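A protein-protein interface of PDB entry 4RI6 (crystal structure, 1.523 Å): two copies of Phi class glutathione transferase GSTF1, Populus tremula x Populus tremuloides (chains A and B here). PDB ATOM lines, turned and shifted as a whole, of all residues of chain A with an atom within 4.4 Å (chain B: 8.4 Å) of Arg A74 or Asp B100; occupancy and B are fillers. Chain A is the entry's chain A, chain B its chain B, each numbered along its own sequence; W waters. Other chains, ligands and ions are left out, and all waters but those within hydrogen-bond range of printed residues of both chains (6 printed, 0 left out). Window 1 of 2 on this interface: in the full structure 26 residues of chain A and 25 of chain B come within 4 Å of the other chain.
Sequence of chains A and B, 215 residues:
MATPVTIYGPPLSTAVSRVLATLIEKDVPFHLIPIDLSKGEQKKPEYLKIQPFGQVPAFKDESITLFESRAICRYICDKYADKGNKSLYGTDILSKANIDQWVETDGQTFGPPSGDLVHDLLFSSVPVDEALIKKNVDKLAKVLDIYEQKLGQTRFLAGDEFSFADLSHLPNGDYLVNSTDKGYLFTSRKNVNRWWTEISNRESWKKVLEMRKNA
The guanidinium group (NE) of Arg A74 lies within salt-bridge range of the side-chain carboxylate (OD2) of Asp B100 (2.8 Å).
OE2 of Glu B104 is in salt-bridge range of NH2 of Arg A74.
OD2 of Asp A100 is in salt-bridge range of NE of Arg B74 (2.7 Å).
NH1 of Arg A74 sits close to NH1 of Arg B74 (3.5 Å).
Water W4 lies within hydrogen-bond range of the side-chain carboxylate (OD2) of Asp B100 and the backbone carbonyl oxygen (O) of Ala A71.
Water W2 lies within hydrogen-bond range of OD2 of Asp A100 (2.8 Å) and O of Ala B71 (2.8 Å).
Water W5 bridges O of Ile B93 (2.8 Å) and OD2 of Asp A78 (3.0 Å).
Water W6 bridges OD1 of Asp A100 (3.3 Å) and NE of Arg B74 (3.5 Å).
Ala A71 touches Asp B100, and with the chains exchanged Asp A100 touches Ala B71.
Arg A74 touches its own counterpart, Arg B74.
Arg A74 touches Asp B100, and with the chains exchanged Asp A100 touches Arg B74.
Of the 13 pairs that touch across the chains among the printed residues, 5 have their exchanged pair printed and touching as well.
Of chain B, only Arg B74 (3.5 Å), Asp B100 (2.8 Å) and Glu B104 (2.6 Å) come within 4 Å of Arg A74.
Asp B100 touches two residues of chain A.
Of the printed residues of chain A, Glu B104 touches Arg A70, Ala A71 and Arg A74.
Printed residues of chain B within 4 Å of Asp A100: Ala B71 (3.4 Å) and Arg B74 (2.7 Å).
Printed residues of chain A within 4 Å of Arg B74: Arg A74 and Asp A100.
Printed residues of chain B within 4 Å of Arg A70: Glu B104 (3.6 Å).
Of the printed residues of chain B, Tyr A75 touches Ile B93, Leu B94 and Ala B97.
Arg B70 touches none of the printed residues of chain A.
Printed residues of chain B that touch a printed residue of chain A: Ala B71, Arg B74, Ile B93, Leu B94, Ala B97, Asp B100, Gln B101 and Glu B104.
Along chain B the printed residues that touch a printed residue of chain A span positions 71 to 104.
Printed residues of chain A that touch a printed residue of chain B: Arg A70, Ala A71, Arg A74, Tyr A75, Asp A78 and Asp A100.
Hydrophobic or aromatic side chains of chain A within 4 Å of the printed part of chain B: Ala A71 and Tyr A75.
Among the printed residues, 13 pairs touch across the chains.
Among the printed residues, pairs that only touch across the chains: Asp A78 with Ile B93 (3.3 Å), Asp A100 with Ala B71 (3.4 Å), Ala A71 with Asp B100 (3.5 Å), Ala A71 with Gln B101 (3.5 Å), Arg A70 with Glu B104 (3.6 Å), Tyr A75 with Leu B94 (3.6 Å), Tyr A75 with Ala B97 (3.7 Å), Tyr A75 with Ile B93 (3.8 Å) and Ala A71 with Glu B104 (3.8 Å).
The side-chain hydroxyl of Tyr A89 lies within hydrogen-bond range of the guanidinium group of Arg A74, at 3.1 Å.
NH1 of Arg A74 is in salt-bridge range of OD1 of Asp A100, at 3.4 Å.
The side-chain carboxylate of Asp B100 sits at hydrogen-bond distance from the side-chain hydroxyl of Tyr B89.
The backbone carbonyl oxygen (O) of Gln B101 lies within hydrogen-bond range of the side-chain hydroxyl (OG1) of Thr B105.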
ATOM      1  N   ARG A  70      17.668   6.562 -21.346  1.00  0.00           N
ATOM      2  CA  ARG A  70      17.353   6.269 -19.960  1.00  0.00           C
ATOM      3  C   ARG A  70      18.339   5.259 -19.365  1.00  0.00           C
ATOM      4  O   ARG A  70      18.619   5.321 -18.178  1.00  0.00           O
ATOM      5  CB  ARG A  70      15.910   5.793 -19.821  1.00  0.00           C
ATOM      6  CG  ARG A  70      14.910   6.875 -20.152  1.00  0.00           C
ATOM      7  CD  ARG A  70      13.507   6.342 -20.330  1.00  0.00           C
ATOM      8  NE  ARG A  70      12.602   7.368 -20.881  1.00  0.00           N
ATOM      9  CZ  ARG A  70      12.503   7.670 -22.173  1.00  0.00           C
ATOM     10  NH1 ARG A  70      13.233   7.033 -23.089  1.00  0.00           N
ATOM     11  NH2 ARG A  70      11.651   8.600 -22.564  1.00  0.00           N
ATOM     12  N   ALA A  71      18.879   4.354 -20.189  1.00  0.00           N
ATOM     13  CA  ALA A  71      19.918   3.419 -19.741  1.00  0.00           C
ATOM     14  C   ALA A  71      21.213   4.160 -19.451  1.00  0.00           C
ATOM     15  O   ALA A  71      21.873   3.939 -18.438  1.00  0.00           O
ATOM     16  CB  ALA A  71      20.157   2.311 -20.794  1.00  0.00           C
ATOM     17  N   ILE A  72      21.558   5.073 -20.341  1.00  0.00           N
ATOM     18  CA  ILE A  72      22.725   5.917 -20.127  1.00  0.00           C
ATOM     19  C   ILE A  72      22.590   6.682 -18.799  1.00  0.00           C
ATOM     20  O   ILE A  72      23.536   6.769 -18.019  1.00  0.00           O
ATOM     21  CB  ILE A  72      22.911   6.899 -21.302  1.00  0.00           C
ATOM     22  CG1 ILE A  72      23.260   6.113 -22.573  1.00  0.00           C
ATOM     23  CG2 ILE A  72      24.013   7.922 -20.996  1.00  0.00           C
ATOM     24  CD1 ILE A  72      23.194   6.905 -23.840  1.00  0.00           C
ATOM     25  N   CYS A  73      21.401   7.211 -18.535  1.00  0.00           N
ATOM     26  CA  CYS A  73      21.210   8.029 -17.345  1.00  0.00           C
ATOM     27  C   CYS A  73      21.261   7.181 -16.085  1.00  0.00           C
ATOM     28  O   CYS A  73      21.802   7.613 -15.075  1.00  0.00           O
ATOM     29  CB  CYS A  73      19.891   8.789 -17.428  1.00  0.00           C
ATOM     30  SG  CYS A  73      19.904  10.114 -18.663  1.00  0.00           S
ATOM     31  N   ARG A  74      20.721   5.962 -16.133  1.00  0.00           N
ATOM     32  CA  ARG A  74      20.810   5.111 -14.960  1.00  0.00           C
ATOM     33  C   ARG A  74      22.269   4.755 -14.667  1.00  0.00           C
ATOM     34  O   ARG A  74      22.681   4.695 -13.520  1.00  0.00           O
ATOM     35  CB  ARG A  74      19.965   3.839 -15.122  1.00  0.00           C
ATOM     36  CG  ARG A  74      18.528   4.064 -14.708  1.00  0.00           C
ATOM     37  CD  ARG A  74      17.708   2.795 -14.601  1.00  0.00           C
ATOM     38  NE  ARG A  74      17.436   2.257 -15.904  1.00  0.00           N
ATOM     39  CZ  ARG A  74      16.345   2.497 -16.631  1.00  0.00           C
ATOM     40  NH1 ARG A  74      15.350   3.245 -16.206  1.00  0.00           N
ATOM     41  NH2 ARG A  74      16.242   1.949 -17.809  1.00  0.00           N
ATOM     42  N   TYR A  75      23.052   4.516 -15.707  1.00  0.00           N
ATOM     43  CA  TYR A  75      24.466   4.207 -15.514  1.00  0.00           C
ATOM     44  C   TYR A  75      25.181   5.388 -14.870  1.00  0.00           C
ATOM     45  O   TYR A  75      25.941   5.227 -13.920  1.00  0.00           O
ATOM     46  CB  TYR A  75      25.126   3.853 -16.843  1.00  0.00           C
ATOM     47  CG  TYR A  75      26.624   3.743 -16.759  1.00  0.00           C
ATOM     48  CD1 TYR A  75      27.218   2.674 -16.096  1.00  0.00           C
ATOM     49  CD2 TYR A  75      27.448   4.704 -17.337  1.00  0.00           C
ATOM     50  CE1 TYR A  75      28.564   2.555 -16.017  1.00  0.00           C
ATOM     51  CE2 TYR A  75      28.812   4.597 -17.256  1.00  0.00           C
ATOM     52  CZ  TYR A  75      29.364   3.520 -16.588  1.00  0.00           C
ATOM     53  OH  TYR A  75      30.725   3.375 -16.500  1.00  0.00           O
ATOM     54  N   ILE A  76      24.917   6.582 -15.385  1.00  0.00           N
ATOM     55  CA  ILE A  76      25.526   7.793 -14.848  1.00  0.00           C
ATOM     56  C   ILE A  76      25.187   7.931 -13.363  1.00  0.00           C
ATOM     57  O   ILE A  76      26.053   8.194 -12.530  1.00  0.00           O
ATOM     58  CB  ILE A  76      25.047   9.034 -15.637  1.00  0.00           C
ATOM     59  CG1 ILE A  76      25.644   9.041 -17.040  1.00  0.00           C
ATOM     60  CG2 ILE A  76      25.422  10.331 -14.914  1.00  0.00           C
ATOM     61  CD1 ILE A  76      25.000  10.017 -17.997  1.00  0.00           C
ATOM     62  N   CYS A  77      23.920   7.739 -13.029  1.00  0.00           N
ATOM     63  CA  CYS A  77      23.487   7.867 -11.649  1.00  0.00           C
ATOM     64  C   CYS A  77      24.123   6.792 -10.749  1.00  0.00           C
ATOM     65  O   CYS A  77      24.448   7.051  -9.580  1.00  0.00           O
ATOM     66  CB  CYS A  77      21.958   7.826 -11.588  1.00  0.00           C
ATOM     67  SG  CYS A  77      21.166   9.342 -12.238  1.00  0.00           S
ATOM     68  N   ASP A  78      24.338   5.606 -11.304  1.00  0.00           N
ATOM     69  CA  ASP A  78      24.967   4.516 -10.567  1.00  0.00           C
ATOM     70  C   ASP A  78      26.462   4.775 -10.355  1.00  0.00           C
ATOM     71  O   ASP A  78      26.969   4.746  -9.226  1.00  0.00           O
ATOM     72  CB  ASP A  78      24.759   3.208 -11.335  1.00  0.00           C
ATOM     73  CG  ASP A  78      24.831   1.979 -10.450  1.00  0.00           C
ATOM     74  OD1 ASP A  78      25.368   2.063  -9.329  1.00  0.00           O
ATOM     75  OD2 ASP A  78      24.363   0.909 -10.901  1.00  0.00           O
ATOM     76  N   TYR A  89      18.306   9.683  -8.479  1.00  0.00           N
ATOM     77  CA  TYR A  89      17.646   8.400  -8.738  1.00  0.00           C
ATOM     78  C   TYR A  89      17.581   7.612  -7.429  1.00  0.00           C
ATOM     79  O   TYR A  89      17.744   6.388  -7.392  1.00  0.00           O
ATOM     80  CB  TYR A  89      18.377   7.624  -9.843  1.00  0.00           C
ATOM     81  CG  TYR A  89      17.471   6.931 -10.861  1.00  0.00           C
ATOM     82  CD1 TYR A  89      16.440   6.085 -10.465  1.00  0.00           C
ATOM     83  CD2 TYR A  89      17.670   7.115 -12.225  1.00  0.00           C
ATOM     84  CE1 TYR A  89      15.636   5.450 -11.400  1.00  0.00           C
ATOM     85  CE2 TYR A  89      16.861   6.504 -13.161  1.00  0.00           C
ATOM     86  CZ  TYR A  89      15.859   5.662 -12.756  1.00  0.00           C
ATOM     87  OH  TYR A  89      15.087   5.047 -13.719  1.00  0.00           O
ATOM     88  N   ASP A 100      11.657   4.960 -10.133  1.00  0.00           N
ATOM     89  CA  ASP A 100      11.732   4.226 -11.389  1.00  0.00           C
ATOM     90  C   ASP A 100      10.352   3.946 -11.997  1.00  0.00           C
ATOM     91  O   ASP A 100      10.202   3.961 -13.228  1.00  0.00           O
ATOM     92  CB  ASP A 100      12.483   2.919 -11.161  1.00  0.00           C
ATOM     93  CG  ASP A 100      12.977   2.281 -12.445  1.00  0.00           C
ATOM     94  OD1 ASP A 100      13.500   2.982 -13.325  1.00  0.00           O
ATOM     95  OD2 ASP A 100      12.856   1.046 -12.563  1.00  0.00           O
ATOM     96  N   VAL A 103       9.638   6.855 -13.960  1.00  0.00           N
ATOM     97  CA  VAL A 103      10.494   6.868 -15.152  1.00  0.00           C
ATOM     98  C   VAL A 103       9.894   5.946 -16.230  1.00  0.00           C
ATOM     99  O   VAL A 103       9.851   6.292 -17.416  1.00  0.00           O
ATOM    100  CB  VAL A 103      11.929   6.446 -14.824  1.00  0.00           C
ATOM    101  CG1 VAL A 103      12.790   6.429 -16.096  1.00  0.00           C
ATOM    102  CG2 VAL A 103      12.538   7.386 -13.784  1.00  0.00           C
ATOM    103  N   ARG B  70       8.411  -3.075 -15.927  1.00  0.00           N
ATOM    104  CA  ARG B  70       9.873  -3.118 -15.909  1.00  0.00           C
ATOM    105  C   ARG B  70      10.447  -2.511 -14.640  1.00  0.00           C
ATOM    106  O   ARG B  70      11.502  -2.933 -14.179  1.00  0.00           O
ATOM    107  CB  ARG B  70      10.452  -2.457 -17.155  1.00  0.00           C
ATOM    108  CG  ARG B  70      10.017  -3.152 -18.429  1.00  0.00           C
ATOM    109  CD  ARG B  70      10.304  -2.333 -19.664  1.00  0.00           C
ATOM    110  NE  ARG B  70       9.766  -2.935 -20.871  1.00  0.00           N
ATOM    111  CZ  ARG B  70       8.507  -2.864 -21.279  1.00  0.00           C
ATOM    112  NH1 ARG B  70       7.578  -2.198 -20.594  1.00  0.00           N
ATOM    113  NH2 ARG B  70       8.179  -3.467 -22.399  1.00  0.00           N
ATOM    114  N   ALA B  71       9.732  -1.567 -14.034  1.00  0.00           N
ATOM    115  CA  ALA B  71      10.142  -1.042 -12.743  1.00  0.00           C
ATOM    116  C   ALA B  71       9.946  -2.090 -11.647  1.00  0.00           C
ATOM    117  O   ALA B  71      10.802  -2.285 -10.799  1.00  0.00           O
ATOM    118  CB  ALA B  71       9.356   0.227 -12.424  1.00  0.00           C
ATOM    119  N   ARG B  74      12.836  -4.505 -12.079  1.00  0.00           N
ATOM    120  CA  ARG B  74      14.123  -3.993 -11.592  1.00  0.00           C
ATOM    121  C   ARG B  74      14.177  -4.032 -10.066  1.00  0.00           C
ATOM    122  O   ARG B  74      15.201  -4.368  -9.488  1.00  0.00           O
ATOM    123  CB  ARG B  74      14.399  -2.561 -12.094  1.00  0.00           C
ATOM    124  CG  ARG B  74      15.065  -2.534 -13.477  1.00  0.00           C
ATOM    125  CD  ARG B  74      15.647  -1.188 -13.854  1.00  0.00           C
ATOM    126  NE  ARG B  74      14.584  -0.293 -14.218  1.00  0.00           N
ATOM    127  CZ  ARG B  74      14.056  -0.183 -15.434  1.00  0.00           C
ATOM    128  NH1 ARG B  74      13.078   0.660 -15.614  1.00  0.00           N
ATOM    129  NH2 ARG B  74      14.487  -0.896 -16.462  1.00  0.00           N
ATOM    130  N   LEU B  88      20.659 -12.268 -13.568  1.00  0.00           N
ATOM    131  CA  LEU B  88      19.574 -11.861 -14.452  1.00  0.00           C
ATOM    132  C   LEU B  88      19.668 -10.408 -14.879  1.00  0.00           C
ATOM    133  O   LEU B  88      19.390 -10.082 -16.018  1.00  0.00           O
ATOM    134  CB  LEU B  88      18.220 -12.093 -13.780  1.00  0.00           C
ATOM    135  CG  LEU B  88      16.997 -11.875 -14.673  1.00  0.00           C
ATOM    136  CD1 LEU B  88      16.945 -12.861 -15.829  1.00  0.00           C
ATOM    137  CD2 LEU B  88      15.745 -12.011 -13.844  1.00  0.00           C
ATOM    138  N   TYR B  89      20.031  -9.529 -13.957  1.00  0.00           N
ATOM    139  CA  TYR B  89      20.184  -8.110 -14.304  1.00  0.00           C
ATOM    140  C   TYR B  89      21.587  -7.651 -13.929  1.00  0.00           C
ATOM    141  O   TYR B  89      21.802  -6.538 -13.446  1.00  0.00           O
ATOM    142  CB  TYR B  89      19.113  -7.269 -13.612  1.00  0.00           C
ATOM    143  CG  TYR B  89      18.507  -6.157 -14.469  1.00  0.00           C
ATOM    144  CD1 TYR B  89      19.297  -5.266 -15.214  1.00  0.00           C
ATOM    145  CD2 TYR B  89      17.133  -6.029 -14.565  1.00  0.00           C
ATOM    146  CE1 TYR B  89      18.716  -4.229 -15.957  1.00  0.00           C
ATOM    147  CE2 TYR B  89      16.550  -5.006 -15.311  1.00  0.00           C
ATOM    148  CZ  TYR B  89      17.348  -4.124 -16.018  1.00  0.00           C
ATOM    149  OH  TYR B  89      16.736  -3.128 -16.741  1.00  0.00           O
ATOM    150  N   GLY B  90      22.547  -8.533 -14.172  1.00  0.00           N
ATOM    151  CA  GLY B  90      23.930  -8.226 -13.901  1.00  0.00           C
ATOM    152  C   GLY B  90      24.308  -8.470 -12.448  1.00  0.00           C
ATOM    153  O   GLY B  90      23.475  -8.841 -11.620  1.00  0.00           O
ATOM    154  N   ILE B  93      27.826  -2.699 -11.563  1.00  0.00           N
ATOM    155  CA  ILE B  93      27.359  -1.526 -12.273  1.00  0.00           C
ATOM    156  C   ILE B  93      27.454  -1.690 -13.791  1.00  0.00           C
ATOM    157  O   ILE B  93      26.509  -1.407 -14.518  1.00  0.00           O
ATOM    158  CB  ILE B  93      28.149  -0.287 -11.812  1.00  0.00           C
ATOM    159  CG1 ILE B  93      27.753   0.048 -10.361  1.00  0.00           C
ATOM    160  CG2 ILE B  93      27.859   0.875 -12.720  1.00  0.00           C
ATOM    161  CD1 ILE B  93      28.549   1.172  -9.699  1.00  0.00           C
ATOM    162  N   LEU B  94      28.579  -2.182 -14.271  1.00  0.00           N
ATOM    163  CA  LEU B  94      28.797  -2.302 -15.701  1.00  0.00           C
ATOM    164  C   LEU B  94      27.948  -3.377 -16.366  1.00  0.00           C
ATOM    165  O   LEU B  94      27.404  -3.159 -17.450  1.00  0.00           O
ATOM    166  CB  LEU B  94      30.275  -2.577 -15.968  1.00  0.00           C
ATOM    167  CG  LEU B  94      31.131  -1.346 -15.674  1.00  0.00           C
ATOM    168  CD1 LEU B  94      32.605  -1.694 -15.559  1.00  0.00           C
ATOM    169  CD2 LEU B  94      30.914  -0.257 -16.719  1.00  0.00           C
ATOM    170  N   SER B  95      27.834  -4.538 -15.738  1.00  0.00           N
ATOM    171  CA  SER B  95      27.086  -5.611 -16.373  1.00  0.00           C
ATOM    172  C   SER B  95      25.599  -5.266 -16.369  1.00  0.00           C
ATOM    173  O   SER B  95      24.862  -5.615 -17.300  1.00  0.00           O
ATOM    174  CB  SER B  95      27.339  -6.950 -15.681  1.00  0.00           C
ATOM    175  OG  SER B  95      27.037  -6.895 -14.302  1.00  0.00           O
ATOM    176  N   LYS B  96      25.159  -4.566 -15.327  1.00  0.00           N
ATOM    177  CA  LYS B  96      23.772  -4.137 -15.233  1.00  0.00           C
ATOM    178  C   LYS B  96      23.436  -3.156 -16.355  1.00  0.00           C
ATOM    179  O   LYS B  96      22.408  -3.294 -17.030  1.00  0.00           O
ATOM    180  CB  LYS B  96      23.509  -3.511 -13.867  1.00  0.00           C
ATOM    181  CG  LYS B  96      22.096  -2.956 -13.690  1.00  0.00           C
ATOM    182  CD  LYS B  96      21.918  -2.196 -12.378  1.00  0.00           C
ATOM    183  CE  LYS B  96      21.603  -3.140 -11.247  1.00  0.00           C
ATOM    184  NZ  LYS B  96      21.438  -2.412  -9.958  1.00  0.00           N
ATOM    185  N   ALA B  97      24.287  -2.159 -16.552  1.00  0.00           N
ATOM    186  CA  ALA B  97      24.028  -1.144 -17.577  1.00  0.00           C
ATOM    187  C   ALA B  97      24.041  -1.757 -18.991  1.00  0.00           C
ATOM    188  O   ALA B  97      23.232  -1.404 -19.853  1.00  0.00           O
ATOM    189  CB  ALA B  97      25.056  -0.016 -17.474  1.00  0.00           C
ATOM    190  N   ASN B  98      24.951  -2.693 -19.218  1.00  0.00           N
ATOM    191  CA  ASN B  98      25.025  -3.354 -20.493  1.00  0.00           C
ATOM    192  C   ASN B  98      23.714  -4.073 -20.825  1.00  0.00           C
ATOM    193  O   ASN B  98      23.241  -4.055 -21.956  1.00  0.00           O
ATOM    194  CB  ASN B  98      26.175  -4.357 -20.505  1.00  0.00           C
ATOM    195  CG  ASN B  98      26.239  -5.119 -21.782  1.00  0.00           C
ATOM    196  OD1 ASN B  98      26.415  -4.537 -22.848  1.00  0.00           O
ATOM    197  ND2 ASN B  98      26.077  -6.441 -21.698  1.00  0.00           N
ATOM    198  N   ILE B  99      23.135  -4.718 -19.826  1.00  0.00           N
ATOM    199  CA  ILE B  99      21.836  -5.329 -20.007  1.00  0.00           C
ATOM    200  C   ILE B  99      20.756  -4.265 -20.191  1.00  0.00           C
ATOM    201  O   ILE B  99      19.890  -4.378 -21.062  1.00  0.00           O
ATOM    202  CB  ILE B  99      21.511  -6.236 -18.818  1.00  0.00           C
ATOM    203  CG1 ILE B  99      22.444  -7.463 -18.834  1.00  0.00           C
ATOM    204  CG2 ILE B  99      20.034  -6.640 -18.837  1.00  0.00           C
ATOM    205  CD1 ILE B  99      22.501  -8.201 -17.510  1.00  0.00           C
ATOM    206  N   ASP B 100      20.829  -3.217 -19.388  1.00  0.00           N
ATOM    207  CA  ASP B 100      19.780  -2.207 -19.338  1.00  0.00           C
ATOM    208  C   ASP B 100      19.539  -1.511 -20.685  1.00  0.00           C
ATOM    209  O   ASP B 100      18.406  -1.167 -21.016  1.00  0.00           O
ATOM    210  CB  ASP B 100      20.139  -1.189 -18.258  1.00  0.00           C
ATOM    211  CG  ASP B 100      18.954  -0.371 -17.783  1.00  0.00           C
ATOM    212  OD1 ASP B 100      17.853  -0.907 -17.596  1.00  0.00           O
ATOM    213  OD2 ASP B 100      19.152   0.834 -17.568  1.00  0.00           O
ATOM    214  N   GLN B 101      20.579  -1.309 -21.487  1.00  0.00           N
ATOM    215  CA  GLN B 101      20.373  -0.630 -22.758  1.00  0.00           C
ATOM    216  C   GLN B 101      19.472  -1.482 -23.665  1.00  0.00           C
ATOM    217  O   GLN B 101      18.692  -0.933 -24.446  1.00  0.00           O
ATOM    218  CB  GLN B 101      21.700  -0.312 -23.457  1.00  0.00           C
ATOM    219  CG  GLN B 101      22.452  -1.524 -23.926  1.00  0.00           C
ATOM    220  CD  GLN B 101      23.913  -1.221 -24.237  1.00  0.00           C
ATOM    221  OE1 GLN B 101      24.241  -0.159 -24.768  1.00  0.00           O
ATOM    222  NE2 GLN B 101      24.788  -2.178 -23.953  1.00  0.00           N
ATOM    223  N   TRP B 102      19.570  -2.806 -23.549  1.00  0.00           N
ATOM    224  CA  TRP B 102      18.735  -3.707 -24.339  1.00  0.00           C
ATOM    225  C   TRP B 102      17.342  -3.848 -23.726  1.00  0.00           C
ATOM    226  O   TRP B 102      16.381  -4.103 -24.432  1.00  0.00           O
ATOM    227  CB  TRP B 102      19.440  -5.071 -24.517  1.00  0.00           C
ATOM    228  CG  TRP B 102      20.627  -4.929 -25.380  1.00  0.00           C
ATOM    229  CD1 TRP B 102      21.928  -4.846 -24.981  1.00  0.00           C
ATOM    230  CD2 TRP B 102      20.630  -4.798 -26.800  1.00  0.00           C
ATOM    231  NE1 TRP B 102      22.753  -4.700 -26.074  1.00  0.00           N
ATOM    232  CE2 TRP B 102      21.977  -4.653 -27.202  1.00  0.00           C
ATOM    233  CE3 TRP B 102      19.625  -4.804 -27.776  1.00  0.00           C
ATOM    234  CZ2 TRP B 102      22.344  -4.505 -28.533  1.00  0.00           C
ATOM    235  CZ3 TRP B 102      19.995  -4.659 -29.111  1.00  0.00           C
ATOM    236  CH2 TRP B 102      21.348  -4.517 -29.471  1.00  0.00           C
ATOM    237  N   VAL B 103      17.222  -3.640 -22.423  1.00  0.00           N
ATOM    238  CA  VAL B 103      15.910  -3.529 -21.798  1.00  0.00           C
ATOM    239  C   VAL B 103      15.195  -2.271 -22.313  1.00  0.00           C
ATOM    240  O   VAL B 103      14.002  -2.305 -22.661  1.00  0.00           O
ATOM    241  CB  VAL B 103      16.007  -3.500 -20.259  1.00  0.00           C
ATOM    242  CG1 VAL B 103      14.611  -3.313 -19.641  1.00  0.00           C
ATOM    243  CG2 VAL B 103      16.649  -4.775 -19.734  1.00  0.00           C
ATOM    244  N   GLU B 104      15.932  -1.169 -22.410  1.00  0.00           N
ATOM    245  CA  GLU B 104      15.364   0.039 -22.987  1.00  0.00           C
ATOM    246  C   GLU B 104      15.023  -0.148 -24.460  1.00  0.00           C
ATOM    247  O   GLU B 104      14.078   0.452 -24.949  1.00  0.00           O
ATOM    248  CB  GLU B 104      16.320   1.217 -22.805  1.00  0.00           C
ATOM    249  CG  GLU B 104      16.392   1.722 -21.370  1.00  0.00           C
ATOM    250  CD  GLU B 104      15.099   2.350 -20.920  1.00  0.00           C
ATOM    251  OE1 GLU B 104      14.504   3.122 -21.701  1.00  0.00           O
ATOM    252  OE2 GLU B 104      14.641   2.045 -19.805  1.00  0.00           O
ATOM    253  N   THR B 105      15.798  -0.969 -25.171  1.00  0.00           N
ATOM    254  CA  THR B 105      15.486  -1.265 -26.550  1.00  0.00           C
ATOM    255  C   THR B 105      14.157  -2.019 -26.622  1.00  0.00           C
ATOM    256  O   THR B 105      13.348  -1.749 -27.511  1.00  0.00           O
ATOM    257  CB  THR B 105      16.640  -2.041 -27.209  1.00  0.00           C
ATOM    258  OG1 THR B 105      17.767  -1.180 -27.280  1.00  0.00           O
ATOM    259  CG2 THR B 105      16.312  -2.479 -28.625  1.00  0.00           C
ATOM    260  N   ASP B 106      13.896  -2.927 -25.691  1.00  0.00           N
ATOM    261  CA  ASP B 106      12.563  -3.506 -25.610  1.00  0.00           C
ATOM    262  C   ASP B 106      11.526  -2.394 -25.406  1.00  0.00           C
ATOM    263  O   ASP B 106      10.537  -2.296 -26.133  1.00  0.00           O
ATOM    264  CB  ASP B 106      12.439  -4.527 -24.482  1.00  0.00           C
ATOM    265  CG  ASP B 106      10.996  -4.935 -24.258  1.00  0.00           C
ATOM    266  OD1 ASP B 106      10.351  -5.306 -25.268  1.00  0.00           O
ATOM    267  OD2 ASP B 106      10.480  -4.853 -23.111  1.00  0.00           O
ATOM    268  N   GLY B 107      11.743  -1.546 -24.417  1.00  0.00           N
ATOM    269  CA  GLY B 107      10.726  -0.565 -24.091  1.00  0.00           C
ATOM    270  C   GLY B 107      10.439   0.477 -25.145  1.00  0.00           C
ATOM    271  O   GLY B 107       9.311   0.942 -25.248  1.00  0.00           O
ATOM    272  N   ALA B 158      22.472  -9.147 -24.940  1.00  0.00           N
ATOM    273  CA  ALA B 158      23.465  -8.316 -24.273  1.00  0.00           C
ATOM    274  C   ALA B 158      24.773  -9.020 -24.036  1.00  0.00           C
ATOM    275  O   ALA B 158      25.700  -8.433 -23.491  1.00  0.00           O
ATOM    276  CB  ALA B 158      22.903  -7.806 -22.937  1.00  0.00           C
ATOM    277  N   SER B 163      19.507 -12.729 -19.947  1.00  0.00           N
ATOM    278  CA  SER B 163      19.338 -11.600 -19.025  1.00  0.00           C
ATOM    279  C   SER B 163      17.919 -11.082 -19.069  1.00  0.00           C
ATOM    280  O   SER B 163      17.094 -11.517 -19.881  1.00  0.00           O
ATOM    281  CB  SER B 163      20.286 -10.463 -19.356  1.00  0.00           C
ATOM    282  OG  SER B 163      19.818  -9.725 -20.464  1.00  0.00           O
ATOM    283  N   PHE B 164      17.649 -10.108 -18.212  1.00  0.00           N
ATOM    284  CA  PHE B 164      16.352  -9.466 -18.233  1.00  0.00           C
ATOM    285  C   PHE B 164      16.048  -8.839 -19.584  1.00  0.00           C
ATOM    286  O   PHE B 164      14.911  -8.722 -19.958  1.00  0.00           O
ATOM    287  CB  PHE B 164      16.237  -8.392 -17.158  1.00  0.00           C
ATOM    288  CG  PHE B 164      14.838  -7.856 -17.033  1.00  0.00           C
ATOM    289  CD1 PHE B 164      13.834  -8.644 -16.496  1.00  0.00           C
ATOM    290  CD2 PHE B 164      14.494  -6.635 -17.543  1.00  0.00           C
ATOM    291  CE1 PHE B 164      12.552  -8.179 -16.426  1.00  0.00           C
ATOM    292  CE2 PHE B 164      13.201  -6.173 -17.458  1.00  0.00           C
ATOM    293  CZ  PHE B 164      12.239  -6.945 -16.916  1.00  0.00           C
ATOM    294  N   ALA B 165      17.061  -8.402 -20.316  1.00  0.00           N
ATOM    295  CA  ALA B 165      16.797  -7.874 -21.647  1.00  0.00           C
ATOM    296  C   ALA B 165      16.096  -8.925 -22.512  1.00  0.00           C
ATOM    297  O   ALA B 165      15.103  -8.627 -23.188  1.00  0.00           O
ATOM    298  CB  ALA B 165      18.082  -7.412 -22.316  1.00  0.00           C
HETATM  299  O   HOH W   1      15.554   5.216 -23.031  1.00  0.00           O
HETATM  300  O   HOH W   2      12.522  -0.186 -10.126  1.00  0.00           O
HETATM  301  O   HOH W   3      12.975   3.509 -18.291  1.00  0.00           O
HETATM  302  O   HOH W   4      21.748   1.436 -17.203  1.00  0.00           O
HETATM  303  O   HOH W   5      24.509   0.476 -13.865  1.00  0.00           O
HETATM  304  O   HOH W   6      16.024   1.614 -11.722  1.00  0.00           O
